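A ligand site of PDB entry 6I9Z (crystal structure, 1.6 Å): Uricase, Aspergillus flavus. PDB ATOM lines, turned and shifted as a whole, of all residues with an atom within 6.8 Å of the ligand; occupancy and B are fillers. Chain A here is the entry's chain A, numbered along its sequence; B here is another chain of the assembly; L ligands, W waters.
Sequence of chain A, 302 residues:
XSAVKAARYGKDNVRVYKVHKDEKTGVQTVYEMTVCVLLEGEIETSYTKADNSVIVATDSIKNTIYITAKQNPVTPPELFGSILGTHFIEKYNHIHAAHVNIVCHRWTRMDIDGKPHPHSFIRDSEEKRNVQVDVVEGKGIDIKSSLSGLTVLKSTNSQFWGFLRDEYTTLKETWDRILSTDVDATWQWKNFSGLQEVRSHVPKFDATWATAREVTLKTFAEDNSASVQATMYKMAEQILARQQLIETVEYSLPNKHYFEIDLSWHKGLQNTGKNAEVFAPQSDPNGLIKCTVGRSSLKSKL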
ATOM      1  N   SER A 158     -19.385  -2.454  -0.190  1.00  0.00           N
ATOM      2  CA  SER A 158     -18.167  -3.113   0.305  1.00  0.00           C
ATOM      3  C   SER A 158     -16.981  -2.386  -0.332  1.00  0.00           C
ATOM      4  O   SER A 158     -17.037  -2.107  -1.525  1.00  0.00           O
ATOM      5  CB  SER A 158     -18.150  -4.595  -0.024  1.00  0.00           C
ATOM      6  OG  SER A 158     -16.891  -5.163   0.286  1.00  0.00           O
ATOM      7  N   GLN A 159     -15.977  -2.107   0.473  1.00  0.00           N
ATOM      8  CA  GLN A 159     -14.754  -1.389   0.062  1.00  0.00           C
ATOM      9  C   GLN A 159     -13.564  -2.190   0.575  1.00  0.00           C
ATOM     10  O   GLN A 159     -13.712  -2.949   1.562  1.00  0.00           O
ATOM     11  CB  GLN A 159     -14.718   0.006   0.700  1.00  0.00           C
ATOM     12  CG  GLN A 159     -16.012   0.768   0.460  1.00  0.00           C
ATOM     13  CD  GLN A 159     -15.992   2.218   0.906  1.00  0.00           C
ATOM     14  OE1 GLN A 159     -14.982   2.749   1.386  1.00  0.00           O
ATOM     15  NE2 GLN A 159     -17.119   2.856   0.718  1.00  0.00           N
ATOM     16  N   PHE A 160     -12.433  -1.936  -0.011  1.00  0.00           N
ATOM     17  CA  PHE A 160     -11.158  -2.452   0.474  1.00  0.00           C
ATOM     18  C   PHE A 160     -10.040  -1.580  -0.074  1.00  0.00           C
ATOM     19  O   PHE A 160      -9.553  -1.775  -1.179  1.00  0.00           O
ATOM     20  CB  PHE A 160     -10.987  -3.963   0.211  1.00  0.00           C
ATOM     21  CG  PHE A 160      -9.828  -4.525   0.988  1.00  0.00           C
ATOM     22  CD1 PHE A 160      -9.850  -4.559   2.364  1.00  0.00           C
ATOM     23  CD2 PHE A 160      -8.705  -5.049   0.361  1.00  0.00           C
ATOM     24  CE1 PHE A 160      -8.783  -5.039   3.098  1.00  0.00           C
ATOM     25  CE2 PHE A 160      -7.651  -5.576   1.090  1.00  0.00           C
ATOM     26  CZ  PHE A 160      -7.662  -5.533   2.474  1.00  0.00           C
ATOM     27  N   PHE A 163      -4.687  -0.859   2.466  1.00  0.00           N
ATOM     28  CA  PHE A 163      -3.880  -2.004   2.911  1.00  0.00           C
ATOM     29  C   PHE A 163      -2.408  -1.803   2.544  1.00  0.00           C
ATOM     30  O   PHE A 163      -2.076  -0.901   1.747  1.00  0.00           O
ATOM     31  CB  PHE A 163      -4.421  -3.322   2.306  1.00  0.00           C
ATOM     32  CG  PHE A 163      -4.641  -3.255   0.827  1.00  0.00           C
ATOM     33  CD1 PHE A 163      -3.611  -3.596  -0.056  1.00  0.00           C
ATOM     34  CD2 PHE A 163      -5.863  -2.893   0.311  1.00  0.00           C
ATOM     35  CE1 PHE A 163      -3.850  -3.551  -1.415  1.00  0.00           C
ATOM     36  CE2 PHE A 163      -6.098  -2.841  -1.053  1.00  0.00           C
ATOM     37  CZ  PHE A 163      -5.064  -3.140  -1.903  1.00  0.00           C
ATOM     38  N   LEU A 171      -2.830  -5.951  -6.084  1.00  0.00           N
ATOM     39  CA  LEU A 171      -4.264  -5.652  -5.895  1.00  0.00           C
ATOM     40  C   LEU A 171      -4.519  -4.137  -5.914  1.00  0.00           C
ATOM     41  O   LEU A 171      -3.821  -3.381  -5.194  1.00  0.00           O
ATOM     42  CB  LEU A 171      -4.689  -6.240  -4.544  1.00  0.00           C
ATOM     43  CG  LEU A 171      -6.169  -6.054  -4.172  1.00  0.00           C
ATOM     44  CD1 LEU A 171      -7.065  -6.833  -5.096  1.00  0.00           C
ATOM     45  CD2 LEU A 171      -6.385  -6.479  -2.730  1.00  0.00           C
ATOM     46  N   ARG A 177     -17.089  -2.918  -4.338  1.00  0.00           N
ATOM     47  CA  ARG A 177     -16.883  -4.296  -4.828  1.00  0.00           C
ATOM     48  C   ARG A 177     -18.059  -5.157  -4.368  1.00  0.00           C
ATOM     49  O   ARG A 177     -18.857  -4.781  -3.499  1.00  0.00           O
ATOM     50  CB  ARG A 177     -15.550  -4.857  -4.338  1.00  0.00           C
ATOM     51  CG  ARG A 177     -15.526  -5.066  -2.835  1.00  0.00           C
ATOM     52  CD  ARG A 177     -14.194  -5.582  -2.334  1.00  0.00           C
ATOM     53  NE  ARG A 177     -14.267  -5.853  -0.903  1.00  0.00           N
ATOM     54  CZ  ARG A 177     -13.413  -6.564  -0.182  1.00  0.00           C
ATOM     55  NH1 ARG A 177     -12.264  -6.998  -0.697  1.00  0.00           N
ATOM     56  NH2 ARG A 177     -13.655  -6.762   1.109  1.00  0.00           N
ATOM     57  N   LEU A 179     -19.148  -8.408  -2.246  1.00  0.00           N
ATOM     58  CA  LEU A 179     -18.726  -9.207  -1.092  1.00  0.00           C
ATOM     59  C   LEU A 179     -19.650 -10.401  -0.964  1.00  0.00           C
ATOM     60  O   LEU A 179     -20.865 -10.246  -0.884  1.00  0.00           O
ATOM     61  CB  LEU A 179     -18.740  -8.335   0.163  1.00  0.00           C
ATOM     62  CG  LEU A 179     -18.266  -9.030   1.436  1.00  0.00           C
ATOM     63  CD1 LEU A 179     -16.856  -9.571   1.278  1.00  0.00           C
ATOM     64  CD2 LEU A 179     -18.319  -8.056   2.603  1.00  0.00           C
ATOM     65  N   SER A 225     -19.028  -1.840   4.371  1.00  0.00           N
ATOM     66  CA  SER A 225     -17.929  -2.671   4.916  1.00  0.00           C
ATOM     67  C   SER A 225     -16.573  -2.109   4.489  1.00  0.00           C
ATOM     68  O   SER A 225     -16.275  -2.014   3.302  1.00  0.00           O
ATOM     69  CB  SER A 225     -18.131  -4.127   4.450  1.00  0.00           C
ATOM     70  OG  SER A 225     -17.007  -4.891   4.779  1.00  0.00           O
ATOM     71  N   ALA A 226     -15.685  -1.940   5.454  1.00  0.00           N
ATOM     72  CA  ALA A 226     -14.300  -1.498   5.254  1.00  0.00           C
ATOM     73  C   ALA A 226     -13.411  -2.685   4.926  1.00  0.00           C
ATOM     74  O   ALA A 226     -12.311  -2.491   4.430  1.00  0.00           O
ATOM     75  CB  ALA A 226     -13.818  -0.810   6.510  1.00  0.00           C
ATOM     76  N   SER A 227     -13.877  -3.893   5.260  1.00  0.00           N
ATOM     77  CA  SER A 227     -13.104  -5.151   5.116  1.00  0.00           C
ATOM     78  C   SER A 227     -14.003  -6.250   5.681  1.00  0.00           C
ATOM     79  O   SER A 227     -14.891  -5.958   6.469  1.00  0.00           O
ATOM     80  CB  SER A 227     -11.750  -5.164   5.806  1.00  0.00           C
ATOM     81  OG  SER A 227     -11.889  -5.100   7.228  1.00  0.00           O
ATOM     82  N   VAL A 228     -13.691  -7.492   5.354  1.00  0.00           N
ATOM     83  CA  VAL A 228     -14.379  -8.605   6.045  1.00  0.00           C
ATOM     84  C   VAL A 228     -14.076  -8.506   7.541  1.00  0.00           C
ATOM     85  O   VAL A 228     -14.985  -8.759   8.335  1.00  0.00           O
ATOM     86  CB  VAL A 228     -13.923  -9.948   5.428  1.00  0.00           C
ATOM     87  CG1 VAL A 228     -14.510 -11.099   6.204  1.00  0.00           C
ATOM     88  CG2 VAL A 228     -14.297 -10.009   3.947  1.00  0.00           C
ATOM     89  N   GLN A 229     -12.819  -8.272   7.880  1.00  0.00           N
ATOM     90  CA  GLN A 229     -12.309  -8.171   9.278  1.00  0.00           C
ATOM     91  C   GLN A 229     -13.242  -7.236  10.068  1.00  0.00           C
ATOM     92  O   GLN A 229     -13.726  -7.589  11.179  1.00  0.00           O
ATOM     93  CB  GLN A 229     -10.873  -7.657   9.275  1.00  0.00           C
ATOM     94  CG  GLN A 229      -9.823  -8.665   8.839  1.00  0.00           C
ATOM     95  CD  GLN A 229      -9.531  -8.691   7.351  1.00  0.00           C
ATOM     96  OE1 GLN A 229     -10.392  -8.379   6.521  1.00  0.00           O
ATOM     97  NE2 GLN A 229      -8.323  -9.173   7.062  1.00  0.00           N
ATOM     98  N   ASN A 255     -13.676 -15.275   1.634  1.00  0.00           N
ATOM     99  CA  ASN A 255     -13.914 -14.105   0.771  1.00  0.00           C
ATOM    100  C   ASN A 255     -14.018 -14.683  -0.641  1.00  0.00           C
ATOM    101  O   ASN A 255     -12.988 -15.075  -1.140  1.00  0.00           O
ATOM    102  CB  ASN A 255     -12.841 -13.044   0.995  1.00  0.00           C
ATOM    103  CG  ASN A 255     -13.199 -11.744   0.299  1.00  0.00           C
ATOM    104  OD1 ASN A 255     -14.262 -11.610  -0.309  1.00  0.00           O
ATOM    105  ND2 ASN A 255     -12.275 -10.791   0.316  1.00  0.00           N
ATOM    106  N   HIS A 257     -14.359 -14.528  -4.270  1.00  0.00           N
ATOM    107  CA  HIS A 257     -14.032 -13.408  -5.169  1.00  0.00           C
ATOM    108  C   HIS A 257     -14.867 -13.458  -6.436  1.00  0.00           C
ATOM    109  O   HIS A 257     -15.059 -14.521  -7.024  1.00  0.00           O
ATOM    110  CB  HIS A 257     -12.543 -13.412  -5.466  1.00  0.00           C
ATOM    111  CG  HIS A 257     -11.697 -13.366  -4.238  1.00  0.00           C
ATOM    112  ND1 HIS A 257     -11.719 -12.285  -3.371  1.00  0.00           N
ATOM    113  CD2 HIS A 257     -10.822 -14.267  -3.732  1.00  0.00           C
ATOM    114  CE1 HIS A 257     -10.849 -12.533  -2.377  1.00  0.00           C
ATOM    115  NE2 HIS A 257     -10.302 -13.745  -2.567  1.00  0.00           N
ATOM    116  N   GLY A 287      -9.911 -15.848  -0.097  1.00  0.00           N
ATOM    117  CA  GLY A 287      -9.525 -15.299   1.200  1.00  0.00           C
ATOM    118  C   GLY A 287     -10.191 -16.111   2.297  1.00  0.00           C
ATOM    119  O   GLY A 287     -11.271 -16.673   2.093  1.00  0.00           O
ATOM    120  N   ILE A 289     -10.774 -15.519   6.494  1.00  0.00           N
ATOM    121  CA  ILE A 289     -10.646 -14.517   7.583  1.00  0.00           C
ATOM    122  C   ILE A 289     -11.291 -15.111   8.830  1.00  0.00           C
ATOM    123  O   ILE A 289     -12.459 -15.483   8.749  1.00  0.00           O
ATOM    124  CB  ILE A 289     -11.322 -13.179   7.204  1.00  0.00           C
ATOM    125  CG1 ILE A 289     -11.049 -12.718   5.769  1.00  0.00           C
ATOM    126  CG2 ILE A 289     -10.900 -12.130   8.232  1.00  0.00           C
ATOM    127  CD1 ILE A 289      -9.654 -12.661   5.434  1.00  0.00           C
ATOM    128  N   TYR B   9      -5.725 -14.743   9.352  1.00  0.00           N
ATOM    129  CA  TYR B   9      -6.341 -14.510   8.034  1.00  0.00           C
ATOM    130  C   TYR B   9      -5.290 -14.833   6.961  1.00  0.00           C
ATOM    131  O   TYR B   9      -4.072 -14.848   7.213  1.00  0.00           O
ATOM    132  CB  TYR B   9      -6.902 -13.099   7.923  1.00  0.00           C
ATOM    133  CG  TYR B   9      -5.814 -12.133   7.550  1.00  0.00           C
ATOM    134  CD1 TYR B   9      -4.797 -11.817   8.431  1.00  0.00           C
ATOM    135  CD2 TYR B   9      -5.684 -11.706   6.244  1.00  0.00           C
ATOM    136  CE1 TYR B   9      -3.691 -11.081   8.019  1.00  0.00           C
ATOM    137  CE2 TYR B   9      -4.618 -10.950   5.824  1.00  0.00           C
ATOM    138  CZ  TYR B   9      -3.609 -10.634   6.721  1.00  0.00           C
ATOM    139  OH  TYR B   9      -2.551  -9.913   6.279  1.00  0.00           O
ATOM    140  N   GLY B  10      -5.783 -15.126   5.766  1.00  0.00           N
ATOM    141  CA  GLY B  10      -4.892 -15.351   4.647  1.00  0.00           C
ATOM    142  C   GLY B  10      -5.622 -15.925   3.442  1.00  0.00           C
ATOM    143  O   GLY B  10      -6.747 -15.539   3.181  1.00  0.00           O
ATOM    144  N   LYS B  11      -4.926 -16.759   2.691  1.00  0.00           N
ATOM    145  CA  LYS B  11      -5.440 -17.270   1.392  1.00  0.00           C
ATOM    146  C   LYS B  11      -5.507 -18.782   1.462  1.00  0.00           C
ATOM    147  O   LYS B  11      -4.532 -19.389   1.884  1.00  0.00           O
ATOM    148  CB  LYS B  11      -4.578 -16.839   0.203  1.00  0.00           C
ATOM    149  CG  LYS B  11      -5.309 -16.858  -1.103  1.00  0.00           C
ATOM    150  CD  LYS B  11      -6.438 -15.887  -1.172  1.00  0.00           C
ATOM    151  CE  LYS B  11      -6.338 -14.877  -2.271  1.00  0.00           C
ATOM    152  NZ  LYS B  11      -7.329 -13.778  -2.133  1.00  0.00           N
ATOM    153  N   ASN B  52      -6.780  -0.799   7.834  1.00  0.00           N
ATOM    154  CA  ASN B  52      -6.249  -1.786   6.850  1.00  0.00           C
ATOM    155  C   ASN B  52      -4.732  -1.690   6.732  1.00  0.00           C
ATOM    156  O   ASN B  52      -4.146  -2.539   6.042  1.00  0.00           O
ATOM    157  CB  ASN B  52      -6.997  -1.701   5.525  1.00  0.00           C
ATOM    158  CG  ASN B  52      -8.438  -2.163   5.633  1.00  0.00           C
ATOM    159  OD1 ASN B  52      -8.778  -2.898   6.574  1.00  0.00           O
ATOM    160  ND2 ASN B  52      -9.305  -1.700   4.742  1.00  0.00           N
ATOM    161  N   ILE B  55      -2.807  -4.835   7.237  1.00  0.00           N
ATOM    162  CA  ILE B  55      -3.172  -6.044   6.420  1.00  0.00           C
ATOM    163  C   ILE B  55      -2.228  -6.200   5.207  1.00  0.00           C
ATOM    164  O   ILE B  55      -2.220  -5.330   4.332  1.00  0.00           O
ATOM    165  CB  ILE B  55      -4.629  -6.004   5.961  1.00  0.00           C
ATOM    166  CG1 ILE B  55      -5.597  -5.989   7.154  1.00  0.00           C
ATOM    167  CG2 ILE B  55      -4.935  -7.221   5.056  1.00  0.00           C
ATOM    168  CD1 ILE B  55      -7.028  -5.787   6.708  1.00  0.00           C
ATOM    169  N   VAL B  56      -1.522  -7.307   5.184  1.00  0.00           N
ATOM    170  CA  VAL B  56      -0.879  -7.880   3.973  1.00  0.00           C
ATOM    171  C   VAL B  56      -2.030  -8.503   3.186  1.00  0.00           C
ATOM    172  O   VAL B  56      -2.657  -9.435   3.739  1.00  0.00           O
ATOM    173  CB  VAL B  56       0.210  -8.876   4.359  1.00  0.00           C
ATOM    174  CG1 VAL B  56       0.806  -9.509   3.108  1.00  0.00           C
ATOM    175  CG2 VAL B  56       1.279  -8.222   5.226  1.00  0.00           C
ATOM    176  N   ALA B  57      -2.436  -7.916   2.069  1.00  0.00           N
ATOM    177  CA  ALA B  57      -3.649  -8.365   1.360  1.00  0.00           C
ATOM    178  C   ALA B  57      -3.543  -9.871   1.084  1.00  0.00           C
ATOM    179  O   ALA B  57      -2.468 -10.363   0.774  1.00  0.00           O
ATOM    180  CB  ALA B  57      -3.870  -7.584   0.095  1.00  0.00           C
ATOM    181  N   THR B  58      -4.670 -10.579   1.141  1.00  0.00           N
ATOM    182  CA  THR B  58      -4.656 -12.042   0.843  1.00  0.00           C
ATOM    183  C   THR B  58      -4.220 -12.236  -0.605  1.00  0.00           C
ATOM    184  O   THR B  58      -3.494 -13.192  -0.864  1.00  0.00           O
ATOM    185  CB  THR B  58      -6.010 -12.688   1.152  1.00  0.00           C
ATOM    186  OG1 THR B  58      -6.991 -12.226   0.229  1.00  0.00           O
ATOM    187  CG2 THR B  58      -6.457 -12.434   2.579  1.00  0.00           C
ATOM    188  N   ASP B  59      -4.576 -11.309  -1.491  1.00  0.00           N
ATOM    189  CA  ASP B  59      -4.106 -11.341  -2.896  1.00  0.00           C
ATOM    190  C   ASP B  59      -2.581 -11.318  -2.930  1.00  0.00           C
ATOM    191  O   ASP B  59      -1.978 -12.040  -3.721  1.00  0.00           O
ATOM    192  CB  ASP B  59      -4.690 -10.178  -3.682  1.00  0.00           C
ATOM    193  CG  ASP B  59      -4.435 -10.351  -5.169  1.00  0.00           C
ATOM    194  OD1 ASP B  59      -5.163 -11.160  -5.767  1.00  0.00           O
ATOM    195  OD2 ASP B  59      -3.457  -9.744  -5.667  1.00  0.00           O
ATOM    196  N   SER B  60      -1.930 -10.529  -2.066  1.00  0.00           N
ATOM    197  CA  SER B  60      -0.447 -10.500  -1.999  1.00  0.00           C
ATOM    198  C   SER B  60       0.111 -11.812  -1.473  1.00  0.00           C
ATOM    199  O   SER B  60       1.207 -12.225  -1.873  1.00  0.00           O
ATOM    200  CB  SER B  60       0.042  -9.320  -1.169  1.00  0.00           C
ATOM    201  OG  SER B  60      -0.600  -8.151  -1.647  1.00  0.00           O
HETATM  202  N1  LIG L   1      -9.818  -8.500   3.638  1.00  0.00           N
HETATM  203  C1  LIG L   1     -10.793  -8.157   2.743  1.00  0.00           C
HETATM  204  O1  LIG L   1     -11.901  -7.831   3.114  1.00  0.00           O
HETATM  205  N2  LIG L   1     -10.489  -8.195   1.402  1.00  0.00           N
HETATM  206  C2  LIG L   1      -9.237  -8.544   1.008  1.00  0.00           C
HETATM  207  C3  LIG L   1      -8.257  -8.839   1.922  1.00  0.00           C
HETATM  208  C4  LIG L   1      -8.522  -8.842   3.323  1.00  0.00           C
HETATM  209  O2  LIG L   1      -7.750  -9.208   4.214  1.00  0.00           O
HETATM  210  N3  LIG L   1      -7.116  -9.123   1.255  1.00  0.00           N
HETATM  211  N4  LIG L   1      -7.354  -8.992  -0.023  1.00  0.00           N
HETATM  212  N5  LIG L   1      -8.622  -8.623  -0.193  1.00  0.00           N
HETATM  213  O   HOH W   1      -9.904  -8.554  -2.616  1.00  0.00           O
HETATM  214  O   HOH W   2      -9.622 -11.912   1.082  1.00  0.00           O
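The guanidinium group of Arg 177 is in hydrogen-bond range of an oxygen (O1) of the ligand (2.9 Å). N of Thr 58 of chain B sits at hydrogen-bond distance from N3 of the ligand, 2.8 Å away. N2 of the ligand lies close to ND2 of Asn 255 (3.3 Å). The side-chain hydroxyl (OG1) of Thr 58 of chain B lies within hydrogen-bond range of a nitrogen (N4) of the ligand (3.3 Å). The backbone NH of Val 228 sits at hydrogen-bond distance from an oxygen (O1) of the ligand (2.9 Å). NE2 of Gln 229 is in hydrogen-bond range of O2 of the ligand, at 2.9 Å.
The backbone carbonyl oxygen of Asn 255 sits at hydrogen-bond distance from a ring nitrogen (NE2) of His 257 (3.3 Å). The backbone carbonyl oxygen (O) of Ser 227 sits at hydrogen-bond distance from the side-chain hydroxyl (OG) of Ser 225. The backbone carbonyl oxygen (O) of Gly 287 is in hydrogen-bond range of the backbone NH (N) of Asn 255 (2.8 Å). O of Val 56 of chain B lies within hydrogen-bond range of OH of Tyr 9 of chain B (2.6 Å). The backbone carbonyl oxygen (O) of Ser 158 sits at hydrogen-bond distance from the backbone NH (N) of Arg 177. OG1 of Thr 58 of chain B is in hydrogen-bond range of NZ of Lys 11 of chain B (2.8 Å). The backbone NH (N) of Gln 229 sits close to the side-chain hydroxyl (OG) of Ser 227 (3.4 Å).
CE2 of Phe 160 touches C2 of the ligand, 3.4 Å away. CD2 of Leu 171 touches N4 of the ligand (3.8 Å). Ser 227 touches the ligand (CA to O1, 3.6 Å). CD2 of Tyr 9 of chain B touches O2 of the ligand, at 3.8 Å. Ile 55 of chain B touches the ligand (CG2 to O2, 3.5 Å). Ala 57 of chain B touches the ligand. Asp 59 of chain B touches the ligand (N to N4, 3.9 Å). Hydrophobic or aromatic side chains within 4 Å of the ligand: Phe 160, Leu 171, Val 228, Tyr 9 of chain B, Ile 55 of chain B and Ala 57 of chain B. Of the 26 residues printed, 12 come within 4 Å of the ligand. The nearest printed residue that does not touch the ligand is Ile 289 (4.1 Å).
Water W1 lies within hydrogen-bond range of a nitrogen (N5) of the ligand and the guanidinium group of Arg 177. Water W2 bridges OG1 of Thr 58 of chain B (2.8 Å) and ND2 of Asn 255 (3.0 Å).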
